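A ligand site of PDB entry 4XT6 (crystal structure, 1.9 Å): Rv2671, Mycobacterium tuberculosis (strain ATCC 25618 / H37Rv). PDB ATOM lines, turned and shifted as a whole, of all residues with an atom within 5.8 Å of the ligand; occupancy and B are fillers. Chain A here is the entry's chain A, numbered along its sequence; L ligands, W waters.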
ATOM      1  N   VAL A  83      20.609 -19.500   2.856  1.00  0.00           N
ATOM      2  CA  VAL A  83      20.068 -20.840   2.647  1.00  0.00           C
ATOM      3  C   VAL A  83      20.756 -21.489   1.452  1.00  0.00           C
ATOM      4  O   VAL A  83      21.080 -20.821   0.476  1.00  0.00           O
ATOM      5  CB  VAL A  83      18.535 -20.753   2.427  1.00  0.00           C
ATOM      6  CG1 VAL A  83      18.209 -19.849   1.260  1.00  0.00           C
ATOM      7  CG2 VAL A  83      17.938 -22.136   2.206  1.00  0.00           C
ATOM      8  N   GLY A  84      21.017 -22.781   1.539  1.00  0.00           N
ATOM      9  CA  GLY A  84      21.628 -23.504   0.440  1.00  0.00           C
ATOM     10  C   GLY A  84      20.566 -23.801  -0.590  1.00  0.00           C
ATOM     11  O   GLY A  84      19.378 -23.796  -0.273  1.00  0.00           O
ATOM     12  N   VAL A  85      20.959 -24.070  -1.834  1.00  0.00           N
ATOM     13  CA  VAL A  85      19.934 -24.183  -2.871  1.00  0.00           C
ATOM     14  C   VAL A  85      19.119 -25.480  -2.815  1.00  0.00           C
ATOM     15  O   VAL A  85      17.982 -25.530  -3.285  1.00  0.00           O
ATOM     16  CB  VAL A  85      20.494 -23.929  -4.280  1.00  0.00           C
ATOM     17  CG1 VAL A  85      21.250 -25.133  -4.781  1.00  0.00           C
ATOM     18  CG2 VAL A  85      19.364 -23.608  -5.209  1.00  0.00           C
ATOM     19  N   GLY A  86      19.690 -26.527  -2.229  1.00  0.00           N
ATOM     20  CA  GLY A  86      18.926 -27.746  -2.017  1.00  0.00           C
ATOM     21  C   GLY A  86      17.672 -27.481  -1.205  1.00  0.00           C
ATOM     22  O   GLY A  86      16.588 -27.994  -1.517  1.00  0.00           O
ATOM     23  N   THR A  87      17.812 -26.655  -0.178  1.00  0.00           N
ATOM     24  CA  THR A  87      16.713 -26.402   0.751  1.00  0.00           C
ATOM     25  C   THR A  87      15.655 -25.443   0.207  1.00  0.00           C
ATOM     26  O   THR A  87      14.522 -25.427   0.698  1.00  0.00           O
ATOM     27  CB  THR A  87      17.228 -25.894   2.106  1.00  0.00           C
ATOM     28  OG1 THR A  87      18.360 -26.682   2.482  1.00  0.00           O
ATOM     29  CG2 THR A  87      16.179 -26.038   3.189  1.00  0.00           C
ATOM     30  N   VAL A  88      16.003 -24.659  -0.821  1.00  0.00           N
ATOM     31  CA  VAL A  88      14.989 -23.793  -1.452  1.00  0.00           C
ATOM     32  C   VAL A  88      14.159 -24.536  -2.506  1.00  0.00           C
ATOM     33  O   VAL A  88      13.465 -23.924  -3.313  1.00  0.00           O
ATOM     34  CB  VAL A  88      15.601 -22.485  -2.052  1.00  0.00           C
ATOM     35  CG1 VAL A  88      16.527 -21.844  -1.046  1.00  0.00           C
ATOM     36  CG2 VAL A  88      16.338 -22.744  -3.361  1.00  0.00           C
ATOM     37  N   ARG A  89      14.230 -25.862  -2.457  1.00  0.00           N
ATOM     38  CA  ARG A  89      13.479 -26.706  -3.394  1.00  0.00           C
ATOM     39  C   ARG A  89      12.643 -27.754  -2.671  1.00  0.00           C
ATOM     40  O   ARG A  89      11.486 -27.511  -2.322  1.00  0.00           O
ATOM     41  CB  ARG A  89      14.449 -27.376  -4.366  1.00  0.00           C
ATOM     42  CG  ARG A  89      15.183 -26.402  -5.271  1.00  0.00           C
ATOM     43  CD  ARG A  89      16.417 -27.037  -5.891  1.00  0.00           C
ATOM     44  NE  ARG A  89      16.960 -26.223  -6.984  1.00  0.00           N
ATOM     45  CZ  ARG A  89      18.187 -26.346  -7.472  1.00  0.00           C
ATOM     46  NH1 ARG A  89      19.022 -27.241  -6.973  1.00  0.00           N
ATOM     47  NH2 ARG A  89      18.594 -25.562  -8.474  1.00  0.00           N
ATOM     48  N   VAL A 120      22.868 -19.792  -1.506  1.00  0.00           N
ATOM     49  CA  VAL A 120      24.212 -20.249  -1.848  1.00  0.00           C
ATOM     50  C   VAL A 120      24.195 -21.345  -2.910  1.00  0.00           C
ATOM     51  O   VAL A 120      23.510 -22.361  -2.753  1.00  0.00           O
ATOM     52  CB  VAL A 120      24.986 -20.750  -0.624  1.00  0.00           C
ATOM     53  CG1 VAL A 120      26.461 -20.970  -0.981  1.00  0.00           C
ATOM     54  CG2 VAL A 120      24.888 -19.728   0.490  1.00  0.00           C
ATOM     55  N   THR A 121      24.920 -21.132  -4.005  1.00  0.00           N
ATOM     56  CA  THR A 121      25.041 -22.124  -5.060  1.00  0.00           C
ATOM     57  C   THR A 121      26.434 -22.111  -5.672  1.00  0.00           C
ATOM     58  O   THR A 121      26.948 -21.070  -6.064  1.00  0.00           O
ATOM     59  CB  THR A 121      23.956 -21.952  -6.151  1.00  0.00           C
ATOM     60  OG1 THR A 121      24.260 -22.807  -7.268  1.00  0.00           O
ATOM     61  CG2 THR A 121      23.877 -20.491  -6.628  1.00  0.00           C
ATOM     62  N   ARG A 122      27.078 -23.269  -5.740  1.00  0.00           N
ATOM     63  CA  ARG A 122      28.394 -23.349  -6.375  1.00  0.00           C
ATOM     64  C   ARG A 122      28.238 -23.350  -7.887  1.00  0.00           C
ATOM     65  O   ARG A 122      29.048 -22.756  -8.619  1.00  0.00           O
ATOM     66  CB  ARG A 122      29.135 -24.623  -5.934  1.00  0.00           C
ATOM     67  CG  ARG A 122      30.607 -24.665  -6.386  1.00  0.00           C
ATOM     68  CD  ARG A 122      31.145 -26.106  -6.429  1.00  0.00           C
ATOM     69  NE  ARG A 122      30.301 -26.936  -7.290  1.00  0.00           N
ATOM     70  CZ  ARG A 122      30.395 -26.966  -8.619  1.00  0.00           C
ATOM     71  NH1 ARG A 122      31.295 -26.205  -9.238  1.00  0.00           N
ATOM     72  NH2 ARG A 122      29.586 -27.733  -9.331  1.00  0.00           N
ATOM     73  N   SER A 123      27.193 -24.005  -8.367  1.00  0.00           N
ATOM     74  CA  SER A 123      26.983 -24.167  -9.808  1.00  0.00           C
ATOM     75  C   SER A 123      26.280 -22.972 -10.442  1.00  0.00           C
ATOM     76  O   SER A 123      26.465 -22.686 -11.628  1.00  0.00           O
ATOM     77  CB  SER A 123      26.161 -25.419 -10.078  1.00  0.00           C
ATOM     78  OG  SER A 123      24.810 -25.217  -9.716  1.00  0.00           O
ATOM     79  N   GLY A 124      25.451 -22.277  -9.666  1.00  0.00           N
ATOM     80  CA  GLY A 124      24.692 -21.153 -10.200  1.00  0.00           C
ATOM     81  C   GLY A 124      23.499 -21.610 -11.000  1.00  0.00           C
ATOM     82  O   GLY A 124      22.800 -20.793 -11.622  1.00  0.00           O
ATOM     83  N   ARG A 125      23.257 -22.917 -11.003  1.00  0.00           N
ATOM     84  CA  ARG A 125      22.183 -23.488 -11.812  1.00  0.00           C
ATOM     85  C   ARG A 125      20.816 -23.292 -11.165  1.00  0.00           C
ATOM     86  O   ARG A 125      20.169 -24.254 -10.745  1.00  0.00           O
ATOM     87  CB  ARG A 125      22.456 -24.982 -12.079  1.00  0.00           C
ATOM     88  CG  ARG A 125      23.636 -25.196 -13.023  1.00  0.00           C
ATOM     89  CD  ARG A 125      24.203 -26.602 -12.913  1.00  0.00           C
ATOM     90  NE  ARG A 125      23.355 -27.617 -13.534  1.00  0.00           N
ATOM     91  CZ  ARG A 125      23.695 -28.324 -14.611  1.00  0.00           C
ATOM     92  NH1 ARG A 125      24.872 -28.140 -15.187  1.00  0.00           N
ATOM     93  NH2 ARG A 125      22.855 -29.227 -15.107  1.00  0.00           N
ATOM     94  N   LEU A 126      20.393 -22.035 -11.091  1.00  0.00           N
ATOM     95  CA  LEU A 126      19.071 -21.674 -10.578  1.00  0.00           C
ATOM     96  C   LEU A 126      18.167 -21.322 -11.745  1.00  0.00           C
ATOM     97  O   LEU A 126      18.607 -20.695 -12.705  1.00  0.00           O
ATOM     98  CB  LEU A 126      19.143 -20.450  -9.651  1.00  0.00           C
ATOM     99  CG  LEU A 126      20.101 -20.460  -8.462  1.00  0.00           C
ATOM    100  CD1 LEU A 126      19.679 -19.459  -7.390  1.00  0.00           C
ATOM    101  CD2 LEU A 126      20.119 -21.839  -7.918  1.00  0.00           C
ATOM    102  N   VAL A 173      33.119 -21.602  -3.710  1.00  0.00           N
ATOM    103  CA  VAL A 173      32.684 -20.616  -2.739  1.00  0.00           C
ATOM    104  C   VAL A 173      33.558 -20.712  -1.483  1.00  0.00           C
ATOM    105  O   VAL A 173      33.758 -21.798  -0.939  1.00  0.00           O
ATOM    106  CB  VAL A 173      31.208 -20.824  -2.339  1.00  0.00           C
ATOM    107  CG1 VAL A 173      30.855 -19.914  -1.184  1.00  0.00           C
ATOM    108  CG2 VAL A 173      30.310 -20.528  -3.530  1.00  0.00           C
ATOM    109  N   GLU A 175      33.698 -19.716   2.287  1.00  0.00           N
ATOM    110  CA  GLU A 175      32.707 -19.336   3.296  1.00  0.00           C
ATOM    111  C   GLU A 175      33.049 -18.012   4.003  1.00  0.00           C
ATOM    112  O   GLU A 175      32.161 -17.189   4.272  1.00  0.00           O
ATOM    113  CB  GLU A 175      32.518 -20.469   4.322  1.00  0.00           C
ATOM    114  CG  GLU A 175      31.675 -21.636   3.829  1.00  0.00           C
ATOM    115  CD  GLU A 175      32.395 -22.541   2.843  1.00  0.00           C
ATOM    116  OE1 GLU A 175      33.657 -22.526   2.828  1.00  0.00           O
ATOM    117  OE2 GLU A 175      31.706 -23.261   2.095  1.00  0.00           O
ATOM    118  N   GLY A 194      19.840 -23.709   7.046  1.00  0.00           N
ATOM    119  CA  GLY A 194      20.200 -24.933   6.342  1.00  0.00           C
ATOM    120  C   GLY A 194      20.432 -24.716   4.875  1.00  0.00           C
ATOM    121  O   GLY A 194      20.559 -23.563   4.431  1.00  0.00           O
ATOM    122  N   GLY A 195      20.481 -25.801   4.109  1.00  0.00           N
ATOM    123  CA  GLY A 195      20.333 -27.148   4.665  1.00  0.00           C
ATOM    124  C   GLY A 195      21.579 -27.772   5.279  1.00  0.00           C
ATOM    125  O   GLY A 195      22.553 -27.080   5.588  1.00  0.00           O
ATOM    126  N   PRO A 196      21.554 -29.107   5.489  1.00  0.00           N
ATOM    127  CA  PRO A 196      22.667 -29.795   6.146  1.00  0.00           C
ATOM    128  C   PRO A 196      23.991 -29.722   5.374  1.00  0.00           C
ATOM    129  O   PRO A 196      25.027 -29.734   6.012  1.00  0.00           O
ATOM    130  CB  PRO A 196      22.189 -31.257   6.262  1.00  0.00           C
ATOM    131  CG  PRO A 196      21.097 -31.377   5.214  1.00  0.00           C
ATOM    132  CD  PRO A 196      20.442 -30.027   5.176  1.00  0.00           C
ATOM    133  N   THR A 197      23.960 -29.672   4.051  1.00  0.00           N
ATOM    134  CA  THR A 197      25.221 -29.542   3.314  1.00  0.00           C
ATOM    135  C   THR A 197      25.873 -28.187   3.600  1.00  0.00           C
ATOM    136  O   THR A 197      27.051 -28.108   3.944  1.00  0.00           O
ATOM    137  CB  THR A 197      24.996 -29.711   1.801  1.00  0.00           C
ATOM    138  OG1 THR A 197      24.427 -31.005   1.546  1.00  0.00           O
ATOM    139  CG2 THR A 197      26.298 -29.577   1.036  1.00  0.00           C
ATOM    140  N   LEU A 198      25.087 -27.113   3.470  1.00  0.00           N
ATOM    141  CA  LEU A 198      25.606 -25.770   3.720  1.00  0.00           C
ATOM    142  C   LEU A 198      26.117 -25.635   5.155  1.00  0.00           C
ATOM    143  O   LEU A 198      27.244 -25.148   5.397  1.00  0.00           O
ATOM    144  CB  LEU A 198      24.520 -24.718   3.435  1.00  0.00           C
ATOM    145  CG  LEU A 198      25.019 -23.278   3.682  1.00  0.00           C
ATOM    146  CD1 LEU A 198      26.177 -22.970   2.765  1.00  0.00           C
ATOM    147  CD2 LEU A 198      23.906 -22.242   3.508  1.00  0.00           C
ATOM    148  N   LEU A 199      25.291 -26.063   6.104  1.00  0.00           N
ATOM    149  CA  LEU A 199      25.711 -25.999   7.500  1.00  0.00           C
ATOM    150  C   LEU A 199      26.991 -26.794   7.690  1.00  0.00           C
ATOM    151  O   LEU A 199      27.886 -26.370   8.413  1.00  0.00           O
ATOM    152  CB  LEU A 199      24.610 -26.508   8.456  1.00  0.00           C
ATOM    153  CG  LEU A 199      25.019 -26.471   9.937  1.00  0.00           C
ATOM    154  CD1 LEU A 199      25.326 -25.066  10.372  1.00  0.00           C
ATOM    155  CD2 LEU A 199      23.968 -27.095  10.865  1.00  0.00           C
ATOM    156  N   THR A 201      29.353 -27.286   5.567  1.00  0.00           N
ATOM    157  CA  THR A 201      30.507 -26.500   5.125  1.00  0.00           C
ATOM    158  C   THR A 201      30.858 -25.360   6.098  1.00  0.00           C
ATOM    159  O   THR A 201      32.037 -25.075   6.308  1.00  0.00           O
ATOM    160  CB  THR A 201      30.326 -25.922   3.700  1.00  0.00           C
ATOM    161  OG1 THR A 201      29.325 -24.912   3.735  1.00  0.00           O
ATOM    162  CG2 THR A 201      29.929 -27.017   2.748  1.00  0.00           C
ATOM    163  N   ARG A 225      18.709 -38.269   8.548  1.00  0.00           N
ATOM    164  CA  ARG A 225      20.035 -37.670   8.498  1.00  0.00           C
ATOM    165  C   ARG A 225      20.225 -36.744   9.691  1.00  0.00           C
ATOM    166  O   ARG A 225      19.266 -36.393  10.357  1.00  0.00           O
ATOM    167  CB  ARG A 225      20.145 -36.850   7.212  1.00  0.00           C
ATOM    168  CG  ARG A 225      19.017 -35.801   7.086  1.00  0.00           C
ATOM    169  CD  ARG A 225      19.373 -34.673   6.104  1.00  0.00           C
ATOM    170  NE  ARG A 225      18.307 -33.673   5.974  1.00  0.00           N
ATOM    171  CZ  ARG A 225      18.216 -32.575   6.736  1.00  0.00           C
ATOM    172  NH1 ARG A 225      19.127 -32.352   7.679  1.00  0.00           N
ATOM    173  NH2 ARG A 225      17.225 -31.700   6.544  1.00  0.00           N
ATOM    174  N   THR A 229      25.545 -32.636   7.124  1.00  0.00           N
ATOM    175  CA  THR A 229      25.990 -33.762   6.311  1.00  0.00           C
ATOM    176  C   THR A 229      27.230 -33.328   5.552  1.00  0.00           C
ATOM    177  O   THR A 229      27.569 -32.141   5.519  1.00  0.00           O
ATOM    178  CB  THR A 229      24.905 -34.257   5.333  1.00  0.00           C
ATOM    179  OG1 THR A 229      24.551 -33.197   4.435  1.00  0.00           O
ATOM    180  CG2 THR A 229      23.662 -34.726   6.088  1.00  0.00           C
HETATM  181  P1  LIG L   1      21.324 -27.510   1.182  1.00  0.00           P
HETATM  182  O1  LIG L   1      22.567 -27.470   2.017  1.00  0.00           O
HETATM  183  O2  LIG L   1      20.483 -26.278   1.419  1.00  0.00           O
HETATM  184  O3  LIG L   1      21.619 -27.685  -0.321  1.00  0.00           O
HETATM  185  C1  LIG L   1      22.865 -27.946  -0.804  1.00  0.00           C
HETATM  186  C2  LIG L   1      23.167 -27.226  -2.103  1.00  0.00           C
HETATM  187  O4  LIG L   1      23.269 -25.776  -1.886  1.00  0.00           O
HETATM  188  C3  LIG L   1      24.434 -27.636  -2.765  1.00  0.00           C
HETATM  189  O5  LIG L   1      24.249 -28.634  -3.688  1.00  0.00           O
HETATM  190  C4  LIG L   1      24.859 -26.413  -3.418  1.00  0.00           C
HETATM  191  O6  LIG L   1      24.144 -26.134  -4.579  1.00  0.00           O
HETATM  192  C5  LIG L   1      24.515 -25.391  -2.363  1.00  0.00           C
HETATM  193  N1  LIG L   1      25.552 -25.298  -1.324  1.00  0.00           N
HETATM  194  C6  LIG L   1      25.513 -25.749  -0.052  1.00  0.00           C
HETATM  195  N2  LIG L   1      26.691 -25.445   0.538  1.00  0.00           N
HETATM  196  C7  LIG L   1      27.477 -24.813  -0.365  1.00  0.00           C
HETATM  197  C8  LIG L   1      28.757 -24.268  -0.358  1.00  0.00           C
HETATM  198  N3  LIG L   1      29.595 -24.309   0.833  1.00  0.00           N
HETATM  199  N4  LIG L   1      29.236 -23.695  -1.478  1.00  0.00           N
HETATM  200  C9  LIG L   1      28.508 -23.617  -2.617  1.00  0.00           C
HETATM  201  N5  LIG L   1      27.269 -24.136  -2.641  1.00  0.00           N
HETATM  202  C10 LIG L   1      26.750 -24.723  -1.546  1.00  0.00           C
HETATM  203  O7  LIG L   1      20.430 -28.732   1.590  1.00  0.00           O
HETATM  204  P2  LIG L   1      20.748 -30.244   1.465  1.00  0.00           P
HETATM  205  O8  LIG L   1      21.935 -30.646   2.277  1.00  0.00           O
HETATM  206  O9  LIG L   1      19.480 -31.038   1.991  1.00  0.00           O
HETATM  207  O10 LIG L   1      20.979 -30.624   0.022  1.00  0.00           O
HETATM  208  P3  LIG L   1      24.724 -26.337  -6.019  1.00  0.00           P
HETATM  209  O11 LIG L   1      26.095 -25.724  -6.127  1.00  0.00           O
HETATM  210  O12 LIG L   1      23.799 -25.671  -7.010  1.00  0.00           O
HETATM  211  O13 LIG L   1      24.815 -27.799  -6.336  1.00  0.00           O
HETATM  212  O   HOH W   1      31.959 -24.224  -3.503  1.00  0.00           O
HETATM  213  O   HOH W   2      22.115 -33.497   2.860  1.00  0.00           O
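The side-chain hydroxyl (OG1) of Thr 201 sits at hydrogen-bond distance from the backbone carbonyl oxygen (O) of Leu 198 (2.7 Å).
OG1 of Thr 121 lies within hydrogen-bond range of N of Ser 123 (3.4 Å).
The backbone NH of Val 120 is in hydrogen-bond range of the backbone carbonyl oxygen of Val 83, 2.9 Å away.
The side-chain hydroxyl (OG1) of Thr 87 sits at hydrogen-bond distance from the backbone NH (N) of Gly 195, 2.8 Å away.
O of Gly 194 lies within hydrogen-bond range of N of Gly 84 (3.0 Å).
The side-chain hydroxyl (OG) of Ser 123 is in hydrogen-bond range of the backbone NH (N) of Arg 125.
The side-chain hydroxyl (OG1) of Thr 201 sits at hydrogen-bond distance from the side-chain carboxylate (OE2) of Glu 175 (3.3 Å).
The backbone NH of Thr 229 is in hydrogen-bond range of the backbone carbonyl oxygen of Pro 196, 3.2 Å away.
The backbone NH (N) of Thr 87 lies within hydrogen-bond range of an oxygen (O2) of the ligand, 3.1 Å away.
The backbone NH of Gly 86 is in hydrogen-bond range of an oxygen (O3) of the ligand (2.9 Å).
The side-chain hydroxyl (OG1) of Thr 201 is in hydrogen-bond range of a nitrogen (N3) of the ligand (3.0 Å).
O8 of the ligand sits at hydrogen-bond distance from N of Thr 197 (2.9 Å).
N of Leu 198 lies within hydrogen-bond range of O1 of the ligand (2.9 Å).
The backbone NH (N) of Arg 122 is in hydrogen-bond range of an oxygen (O11) of the ligand (2.7 Å).
The backbone NH of Ser 123 sits at hydrogen-bond distance from an oxygen (O11) of the ligand.
O12 of the ligand lies within hydrogen-bond range of OG1 of Thr 121 (2.9 Å).
The side-chain hydroxyl (OG1) of Thr 197 sits at hydrogen-bond distance from an oxygen (O8) of the ligand (2.6 Å).
The side-chain carboxylate (OE2) of Glu 175 sits at hydrogen-bond distance from a nitrogen (N3) of the ligand, 2.7 Å away.
An oxygen (O2) of the ligand is in hydrogen-bond range of the backbone NH (N) of Gly 195, 2.7 Å away.
An oxygen (O12) of the ligand lies within hydrogen-bond range of the side-chain hydroxyl (OG) of Ser 123 (2.9 Å).
OG1 of Thr 87 is in hydrogen-bond range of O2 of the ligand (2.4 Å).
The backbone NH (N) of Val 85 is in hydrogen-bond range of an oxygen (O4) of the ligand (2.9 Å).
The backbone carbonyl oxygen (O) of Gly 84 sits close to an oxygen (O2) of the ligand (3.2 Å).
Val 120 touches the ligand.
Val 173 touches the ligand (CB to N4, 3.6 Å).
C of Gly 194 touches O2 of the ligand (3.8 Å).
Pro 196 touches the ligand.
The nearest printed residue that does not touch the ligand is Thr 229 (4.2 Å).
Water W2 lies within hydrogen-bond range of O8 of the ligand (2.9 Å) and OG1 of Thr 229 (2.9 Å).
Water W1 lies within hydrogen-bond range of the backbone NH (N) of Val 173 (2.9 Å) and a nitrogen (N4) of the ligand (3.4 Å).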
